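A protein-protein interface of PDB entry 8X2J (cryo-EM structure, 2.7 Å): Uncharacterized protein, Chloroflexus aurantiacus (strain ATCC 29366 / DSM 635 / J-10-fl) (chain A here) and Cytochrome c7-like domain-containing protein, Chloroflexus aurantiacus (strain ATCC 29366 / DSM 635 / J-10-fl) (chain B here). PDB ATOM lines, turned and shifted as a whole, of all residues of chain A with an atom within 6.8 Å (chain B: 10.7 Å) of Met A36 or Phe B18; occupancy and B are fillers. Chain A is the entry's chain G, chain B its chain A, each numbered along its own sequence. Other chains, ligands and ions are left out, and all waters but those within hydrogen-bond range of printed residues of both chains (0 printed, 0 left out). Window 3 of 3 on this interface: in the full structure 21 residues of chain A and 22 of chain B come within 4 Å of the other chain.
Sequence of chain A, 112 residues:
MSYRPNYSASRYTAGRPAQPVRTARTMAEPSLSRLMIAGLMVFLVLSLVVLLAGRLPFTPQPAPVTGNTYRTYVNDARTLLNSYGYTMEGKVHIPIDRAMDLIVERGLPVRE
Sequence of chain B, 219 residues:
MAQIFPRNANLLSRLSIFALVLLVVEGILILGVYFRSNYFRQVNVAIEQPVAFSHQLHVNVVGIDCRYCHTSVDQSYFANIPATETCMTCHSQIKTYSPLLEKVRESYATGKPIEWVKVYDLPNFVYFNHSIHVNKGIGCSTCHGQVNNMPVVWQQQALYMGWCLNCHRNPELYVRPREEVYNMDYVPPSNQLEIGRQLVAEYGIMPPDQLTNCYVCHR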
ATOM      1  N   LEU A  32       1.216  28.030 -14.572  1.00  0.00           N
ATOM      2  CA  LEU A  32       1.718  29.278 -15.129  1.00  0.00           C
ATOM      3  C   LEU A  32       2.189  29.064 -16.560  1.00  0.00           C
ATOM      4  O   LEU A  32       2.989  28.171 -16.831  1.00  0.00           O
ATOM      5  CB  LEU A  32       2.851  29.838 -14.270  1.00  0.00           C
ATOM      6  CG  LEU A  32       3.314  31.264 -14.575  1.00  0.00           C
ATOM      7  CD1 LEU A  32       2.134  32.218 -14.645  1.00  0.00           C
ATOM      8  CD2 LEU A  32       4.318  31.734 -13.534  1.00  0.00           C
ATOM      9  N   SER A  33       1.679  29.895 -17.472  1.00  0.00           N
ATOM     10  CA  SER A  33       2.009  29.775 -18.887  1.00  0.00           C
ATOM     11  C   SER A  33       3.434  30.206 -19.200  1.00  0.00           C
ATOM     12  O   SER A  33       3.992  29.758 -20.206  1.00  0.00           O
ATOM     13  CB  SER A  33       1.036  30.606 -19.719  1.00  0.00           C
ATOM     14  OG  SER A  33       1.300  31.987 -19.557  1.00  0.00           O
ATOM     15  N   ARG A  34       4.024  31.076 -18.374  1.00  0.00           N
ATOM     16  CA  ARG A  34       5.390  31.529 -18.619  1.00  0.00           C
ATOM     17  C   ARG A  34       6.392  30.401 -18.416  1.00  0.00           C
ATOM     18  O   ARG A  34       7.382  30.302 -19.151  1.00  0.00           O
ATOM     19  CB  ARG A  34       5.719  32.714 -17.713  1.00  0.00           C
ATOM     20  CG  ARG A  34       5.323  34.057 -18.300  1.00  0.00           C
ATOM     21  CD  ARG A  34       4.922  35.041 -17.217  1.00  0.00           C
ATOM     22  NE  ARG A  34       5.164  36.422 -17.619  1.00  0.00           N
ATOM     23  CZ  ARG A  34       6.317  37.057 -17.462  1.00  0.00           C
ATOM     24  NH1 ARG A  34       7.366  36.461 -16.920  1.00  0.00           N
ATOM     25  NH2 ARG A  34       6.419  38.322 -17.858  1.00  0.00           N
ATOM     26  N   LEU A  35       6.146  29.533 -17.434  1.00  0.00           N
ATOM     27  CA  LEU A  35       7.002  28.367 -17.252  1.00  0.00           C
ATOM     28  C   LEU A  35       6.819  27.358 -18.380  1.00  0.00           C
ATOM     29  O   LEU A  35       7.783  26.690 -18.766  1.00  0.00           O
ATOM     30  CB  LEU A  35       6.729  27.722 -15.894  1.00  0.00           C
ATOM     31  CG  LEU A  35       7.502  28.360 -14.738  1.00  0.00           C
ATOM     32  CD1 LEU A  35       7.046  27.807 -13.403  1.00  0.00           C
ATOM     33  CD2 LEU A  35       8.999  28.170 -14.918  1.00  0.00           C
ATOM     34  N   MET A  36       5.603  27.256 -18.931  1.00  0.00           N
ATOM     35  CA  MET A  36       5.381  26.446 -20.128  1.00  0.00           C
ATOM     36  C   MET A  36       6.161  26.991 -21.318  1.00  0.00           C
ATOM     37  O   MET A  36       6.750  26.223 -22.086  1.00  0.00           O
ATOM     38  CB  MET A  36       3.891  26.394 -20.468  1.00  0.00           C
ATOM     39  CG  MET A  36       2.973  26.016 -19.324  1.00  0.00           C
ATOM     40  SD  MET A  36       2.670  24.246 -19.205  1.00  0.00           S
ATOM     41  CE  MET A  36       1.593  24.182 -17.776  1.00  0.00           C
ATOM     42  N   ILE A  37       6.185  28.317 -21.475  1.00  0.00           N
ATOM     43  CA  ILE A  37       6.916  28.944 -22.574  1.00  0.00           C
ATOM     44  C   ILE A  37       8.421  28.749 -22.408  1.00  0.00           C
ATOM     45  O   ILE A  37       9.128  28.435 -23.374  1.00  0.00           O
ATOM     46  CB  ILE A  37       6.524  30.433 -22.672  1.00  0.00           C
ATOM     47  CG1 ILE A  37       5.111  30.566 -23.241  1.00  0.00           C
ATOM     48  CG2 ILE A  37       7.503  31.228 -23.525  1.00  0.00           C
ATOM     49  CD1 ILE A  37       4.942  29.940 -24.608  1.00  0.00           C
ATOM     50  N   ALA A  38       8.927  28.893 -21.178  1.00  0.00           N
ATOM     51  CA  ALA A  38      10.351  28.686 -20.918  1.00  0.00           C
ATOM     52  C   ALA A  38      10.759  27.229 -21.121  1.00  0.00           C
ATOM     53  O   ALA A  38      11.831  26.952 -21.676  1.00  0.00           O
ATOM     54  CB  ALA A  38      10.698  29.147 -19.504  1.00  0.00           C
ATOM     55  N   GLY A  39       9.916  26.286 -20.689  1.00  0.00           N
ATOM     56  CA  GLY A  39      10.201  24.881 -20.930  1.00  0.00           C
ATOM     57  C   GLY A  39      10.144  24.513 -22.400  1.00  0.00           C
ATOM     58  O   GLY A  39      10.936  23.694 -22.873  1.00  0.00           O
ATOM     59  N   LEU A  40       9.217  25.124 -23.147  1.00  0.00           N
ATOM     60  CA  LEU A  40       9.153  24.915 -24.589  1.00  0.00           C
ATOM     61  C   LEU A  40      10.381  25.491 -25.288  1.00  0.00           C
ATOM     62  O   LEU A  40      10.889  24.895 -26.243  1.00  0.00           O
ATOM     63  CB  LEU A  40       7.869  25.531 -25.145  1.00  0.00           C
ATOM     64  CG  LEU A  40       7.702  25.641 -26.661  1.00  0.00           C
ATOM     65  CD1 LEU A  40       7.693  24.264 -27.302  1.00  0.00           C
ATOM     66  CD2 LEU A  40       6.441  26.412 -27.004  1.00  0.00           C
ATOM     67  N   MET A  41      10.874  26.642 -24.821  1.00  0.00           N
ATOM     68  CA  MET A  41      12.088  27.223 -25.390  1.00  0.00           C
ATOM     69  C   MET A  41      13.310  26.359 -25.105  1.00  0.00           C
ATOM     70  O   MET A  41      14.169  26.184 -25.979  1.00  0.00           O
ATOM     71  CB  MET A  41      12.297  28.639 -24.851  1.00  0.00           C
ATOM     72  CG  MET A  41      11.393  29.684 -25.484  1.00  0.00           C
ATOM     73  SD  MET A  41      11.531  29.731 -27.281  1.00  0.00           S
ATOM     74  CE  MET A  41       9.876  29.239 -27.763  1.00  0.00           C
ATOM     75  N   ALA B   9       2.228  23.045  -5.493  1.00  0.00           N
ATOM     76  CA  ALA B   9       2.054  21.683  -5.983  1.00  0.00           C
ATOM     77  C   ALA B   9       1.223  21.634  -7.258  1.00  0.00           C
ATOM     78  O   ALA B   9       1.432  20.745  -8.088  1.00  0.00           O
ATOM     79  CB  ALA B   9       1.417  20.810  -4.904  1.00  0.00           C
ATOM     80  N   ASN B  10       0.291  22.577  -7.440  1.00  0.00           N
ATOM     81  CA  ASN B  10      -0.515  22.610  -8.660  1.00  0.00           C
ATOM     82  C   ASN B  10       0.335  22.966  -9.872  1.00  0.00           C
ATOM     83  O   ASN B  10       0.274  22.292 -10.911  1.00  0.00           O
ATOM     84  CB  ASN B  10      -1.655  23.613  -8.508  1.00  0.00           C
ATOM     85  CG  ASN B  10      -2.353  23.495  -7.181  1.00  0.00           C
ATOM     86  OD1 ASN B  10      -2.421  22.415  -6.610  1.00  0.00           O
ATOM     87  ND2 ASN B  10      -2.887  24.604  -6.686  1.00  0.00           N
ATOM     88  N   LEU B  11       1.136  24.028  -9.746  1.00  0.00           N
ATOM     89  CA  LEU B  11       2.073  24.413 -10.794  1.00  0.00           C
ATOM     90  C   LEU B  11       3.116  23.333 -11.027  1.00  0.00           C
ATOM     91  O   LEU B  11       3.487  23.071 -12.175  1.00  0.00           O
ATOM     92  CB  LEU B  11       2.739  25.740 -10.423  1.00  0.00           C
ATOM     93  CG  LEU B  11       3.950  26.232 -11.215  1.00  0.00           C
ATOM     94  CD1 LEU B  11       3.582  26.479 -12.663  1.00  0.00           C
ATOM     95  CD2 LEU B  11       4.511  27.492 -10.582  1.00  0.00           C
ATOM     96  N   LEU B  12       3.568  22.674  -9.954  1.00  0.00           N
ATOM     97  CA  LEU B  12       4.537  21.592 -10.085  1.00  0.00           C
ATOM     98  C   LEU B  12       3.950  20.396 -10.827  1.00  0.00           C
ATOM     99  O   LEU B  12       4.628  19.791 -11.659  1.00  0.00           O
ATOM    100  CB  LEU B  12       5.037  21.178  -8.703  1.00  0.00           C
ATOM    101  CG  LEU B  12       6.396  20.486  -8.659  1.00  0.00           C
ATOM    102  CD1 LEU B  12       7.476  21.444  -9.125  1.00  0.00           C
ATOM    103  CD2 LEU B  12       6.689  19.980  -7.256  1.00  0.00           C
ATOM    104  N   SER B  13       2.683  20.061 -10.568  1.00  0.00           N
ATOM    105  CA  SER B  13       2.050  18.931 -11.244  1.00  0.00           C
ATOM    106  C   SER B  13       1.772  19.235 -12.711  1.00  0.00           C
ATOM    107  O   SER B  13       1.966  18.369 -13.577  1.00  0.00           O
ATOM    108  CB  SER B  13       0.758  18.556 -10.524  1.00  0.00           C
ATOM    109  OG  SER B  13       1.032  18.107  -9.212  1.00  0.00           O
ATOM    110  N   ARG B  14       1.313  20.456 -13.008  1.00  0.00           N
ATOM    111  CA  ARG B  14       1.082  20.845 -14.398  1.00  0.00           C
ATOM    112  C   ARG B  14       2.389  20.901 -15.183  1.00  0.00           C
ATOM    113  O   ARG B  14       2.461  20.425 -16.325  1.00  0.00           O
ATOM    114  CB  ARG B  14       0.368  22.191 -14.450  1.00  0.00           C
ATOM    115  CG  ARG B  14      -1.085  22.127 -14.034  1.00  0.00           C
ATOM    116  CD  ARG B  14      -1.532  23.443 -13.438  1.00  0.00           C
ATOM    117  NE  ARG B  14      -2.631  23.273 -12.498  1.00  0.00           N
ATOM    118  CZ  ARG B  14      -3.104  24.240 -11.724  1.00  0.00           C
ATOM    119  NH1 ARG B  14      -2.583  25.455 -11.740  1.00  0.00           N
ATOM    120  NH2 ARG B  14      -4.125  23.980 -10.913  1.00  0.00           N
ATOM    121  N   LEU B  15       3.443  21.445 -14.567  1.00  0.00           N
ATOM    122  CA  LEU B  15       4.752  21.482 -15.202  1.00  0.00           C
ATOM    123  C   LEU B  15       5.352  20.087 -15.325  1.00  0.00           C
ATOM    124  O   LEU B  15       6.102  19.825 -16.266  1.00  0.00           O
ATOM    125  CB  LEU B  15       5.676  22.407 -14.409  1.00  0.00           C
ATOM    126  CG  LEU B  15       7.030  22.797 -14.999  1.00  0.00           C
ATOM    127  CD1 LEU B  15       6.841  23.573 -16.290  1.00  0.00           C
ATOM    128  CD2 LEU B  15       7.826  23.613 -13.995  1.00  0.00           C
ATOM    129  N   SER B  16       5.008  19.175 -14.410  1.00  0.00           N
ATOM    130  CA  SER B  16       5.464  17.794 -14.514  1.00  0.00           C
ATOM    131  C   SER B  16       4.802  17.070 -15.678  1.00  0.00           C
ATOM    132  O   SER B  16       5.465  16.311 -16.392  1.00  0.00           O
ATOM    133  CB  SER B  16       5.191  17.057 -13.204  1.00  0.00           C
ATOM    134  OG  SER B  16       5.964  15.875 -13.113  1.00  0.00           O
ATOM    135  N   ILE B  17       3.498  17.291 -15.882  1.00  0.00           N
ATOM    136  CA  ILE B  17       2.804  16.709 -17.036  1.00  0.00           C
ATOM    137  C   ILE B  17       3.368  17.273 -18.339  1.00  0.00           C
ATOM    138  O   ILE B  17       3.630  16.528 -19.300  1.00  0.00           O
ATOM    139  CB  ILE B  17       1.285  16.953 -16.917  1.00  0.00           C
ATOM    140  CG1 ILE B  17       0.703  16.184 -15.728  1.00  0.00           C
ATOM    141  CG2 ILE B  17       0.555  16.586 -18.206  1.00  0.00           C
ATOM    142  CD1 ILE B  17       0.607  14.688 -15.939  1.00  0.00           C
ATOM    143  N   PHE B  18       3.598  18.591 -18.370  1.00  0.00           N
ATOM    144  CA  PHE B  18       4.182  19.250 -19.538  1.00  0.00           C
ATOM    145  C   PHE B  18       5.589  18.739 -19.835  1.00  0.00           C
ATOM    146  O   PHE B  18       5.924  18.453 -20.992  1.00  0.00           O
ATOM    147  CB  PHE B  18       4.199  20.759 -19.299  1.00  0.00           C
ATOM    148  CG  PHE B  18       4.515  21.569 -20.515  1.00  0.00           C
ATOM    149  CD1 PHE B  18       3.678  21.544 -21.617  1.00  0.00           C
ATOM    150  CD2 PHE B  18       5.643  22.374 -20.546  1.00  0.00           C
ATOM    151  CE1 PHE B  18       3.965  22.299 -22.733  1.00  0.00           C
ATOM    152  CE2 PHE B  18       5.935  23.133 -21.660  1.00  0.00           C
ATOM    153  CZ  PHE B  18       5.096  23.095 -22.755  1.00  0.00           C
ATOM    154  N   ALA B  19       6.413  18.583 -18.795  1.00  0.00           N
ATOM    155  CA  ALA B  19       7.775  18.099 -18.971  1.00  0.00           C
ATOM    156  C   ALA B  19       7.810  16.625 -19.342  1.00  0.00           C
ATOM    157  O   ALA B  19       8.712  16.204 -20.064  1.00  0.00           O
ATOM    158  CB  ALA B  19       8.587  18.347 -17.701  1.00  0.00           C
ATOM    159  N   LEU B  20       6.840  15.833 -18.879  1.00  0.00           N
ATOM    160  CA  LEU B  20       6.777  14.431 -19.280  1.00  0.00           C
ATOM    161  C   LEU B  20       6.411  14.288 -20.752  1.00  0.00           C
ATOM    162  O   LEU B  20       6.996  13.458 -21.464  1.00  0.00           O
ATOM    163  CB  LEU B  20       5.777  13.680 -18.401  1.00  0.00           C
ATOM    164  CG  LEU B  20       5.727  12.162 -18.569  1.00  0.00           C
ATOM    165  CD1 LEU B  20       6.984  11.520 -18.008  1.00  0.00           C
ATOM    166  CD2 LEU B  20       4.485  11.591 -17.907  1.00  0.00           C
ATOM    167  N   VAL B  21       5.459  15.098 -21.229  1.00  0.00           N
ATOM    168  CA  VAL B  21       5.103  15.077 -22.650  1.00  0.00           C
ATOM    169  C   VAL B  21       6.276  15.557 -23.506  1.00  0.00           C
ATOM    170  O   VAL B  21       6.613  14.941 -24.530  1.00  0.00           O
ATOM    171  CB  VAL B  21       3.829  15.911 -22.890  1.00  0.00           C
ATOM    172  CG1 VAL B  21       3.566  16.105 -24.377  1.00  0.00           C
ATOM    173  CG2 VAL B  21       2.635  15.242 -22.233  1.00  0.00           C
ATOM    174  N   LEU B  22       6.946  16.634 -23.072  1.00  0.00           N
ATOM    175  CA  LEU B  22       8.123  17.132 -23.780  1.00  0.00           C
ATOM    176  C   LEU B  22       9.278  16.138 -23.747  1.00  0.00           C
ATOM    177  O   LEU B  22      10.037  16.048 -24.713  1.00  0.00           O
ATOM    178  CB  LEU B  22       8.571  18.466 -23.184  1.00  0.00           C
ATOM    179  CG  LEU B  22       7.783  19.715 -23.573  1.00  0.00           C
ATOM    180  CD1 LEU B  22       8.493  20.953 -23.066  1.00  0.00           C
ATOM    181  CD2 LEU B  22       7.590  19.789 -25.073  1.00  0.00           C
ATOM    182  N   LEU B  23       9.406  15.369 -22.665  1.00  0.00           N
ATOM    183  CA  LEU B  23      10.471  14.378 -22.564  1.00  0.00           C
ATOM    184  C   LEU B  23      10.204  13.187 -23.474  1.00  0.00           C
ATOM    185  O   LEU B  23      11.139  12.630 -24.058  1.00  0.00           O
ATOM    186  CB  LEU B  23      10.617  13.930 -21.111  1.00  0.00           C
ATOM    187  CG  LEU B  23      12.003  13.492 -20.646  1.00  0.00           C
ATOM    188  CD1 LEU B  23      12.915  14.698 -20.503  1.00  0.00           C
ATOM    189  CD2 LEU B  23      11.901  12.732 -19.336  1.00  0.00           C
ATOM    190  N   VAL B  24       8.935  12.786 -23.608  1.00  0.00           N
ATOM    191  CA  VAL B  24       8.575  11.722 -24.548  1.00  0.00           C
ATOM    192  C   VAL B  24       8.847  12.159 -25.986  1.00  0.00           C
ATOM    193  O   VAL B  24       9.422  11.402 -26.787  1.00  0.00           O
ATOM    194  CB  VAL B  24       7.103  11.312 -24.336  1.00  0.00           C
ATOM    195  CG1 VAL B  24       6.571  10.507 -25.511  1.00  0.00           C
ATOM    196  CG2 VAL B  24       6.960  10.522 -23.048  1.00  0.00           C
ATOM    197  N   VAL B  25       8.474  13.402 -26.318  1.00  0.00           N
ATOM    198  CA  VAL B  25       8.719  13.941 -27.658  1.00  0.00           C
ATOM    199  C   VAL B  25      10.219  14.065 -27.928  1.00  0.00           C
ATOM    200  O   VAL B  25      10.698  13.721 -29.016  1.00  0.00           O
ATOM    201  CB  VAL B  25       7.983  15.286 -27.825  1.00  0.00           C
ATOM    202  CG1 VAL B  25       8.418  16.014 -29.089  1.00  0.00           C
ATOM    203  CG2 VAL B  25       6.481  15.058 -27.852  1.00  0.00           C
ATOM    204  N   GLU B  26      10.987  14.501 -26.924  1.00  0.00           N
ATOM    205  CA  GLU B  26      12.433  14.633 -27.074  1.00  0.00           C
ATOM    206  C   GLU B  26      13.116  13.276 -27.203  1.00  0.00           C
ATOM    207  O   GLU B  26      14.101  13.146 -27.934  1.00  0.00           O
ATOM    208  CB  GLU B  26      13.007  15.409 -25.888  1.00  0.00           C
ATOM    209  CG  GLU B  26      14.460  15.813 -26.040  1.00  0.00           C
ATOM    210  CD  GLU B  26      14.696  16.687 -27.253  1.00  0.00           C
ATOM    211  OE1 GLU B  26      14.130  17.796 -27.304  1.00  0.00           O
ATOM    212  OE2 GLU B  26      15.457  16.270 -28.150  1.00  0.00           O
ATOM    213  N   GLY B  27      12.612  12.254 -26.508  1.00  0.00           N
ATOM    214  CA  GLY B  27      13.167  10.919 -26.664  1.00  0.00           C
ATOM    215  C   GLY B  27      12.910  10.328 -28.037  1.00  0.00           C
ATOM    216  O   GLY B  27      13.808   9.721 -28.637  1.00  0.00           O
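Among the printed residues, merely in contact across the chains: Met A36 with Phe B18 (3.2 Å), Leu A32 with Leu B11 (3.4 Å), Gly A39 with Leu B22 (3.7 Å) and Leu A35 with Leu B11 (3.8 Å).
Met A36 touches just one residue of chain B: Phe B18 (3.2 Å).
Of chain A, only Met A36 comes within 4 Å of Phe B18.
Ser A33 touches none of the printed residues of chain B.
Leu A35 touches just one residue of chain B: Leu B11.
No residue of chain B comes within 4 Å of Ile A37.
No residue of chain B comes within 4 Å of Ala A38.
Of chain B, only Leu B22 comes within 4 Å of Gly A39.
Printed residues of chain A within 4 Å of Leu B22: Gly A39.
Printed residues of chain B within 4 Å of Leu A32: Leu B11.
Printed residues of chain A within 4 Å of Leu B11: Leu A32 (3.4 Å) and Leu A35 (3.8 Å).
The nearest residue of chain B that does not touch Met A36 is Arg B14 (4.1 Å).
The nearest printed residue of chain A that does not touch Leu B11 is Met A36 (5.9 Å).
Hydrophobic or aromatic side chains of chain B that line the printed part of chain A: Leu B11, Phe B18 and Leu B22.
Printed residues of chain A that touch a printed residue of chain B: Leu A32, Leu A35, Met A36 and Gly A39.
Hydrophobic or aromatic side chains of chain A that line the printed part of chain B: Leu A32, Leu A35 and Met A36.
Along chain A the printed residues that touch a printed residue of chain B span positions 32 to 39.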
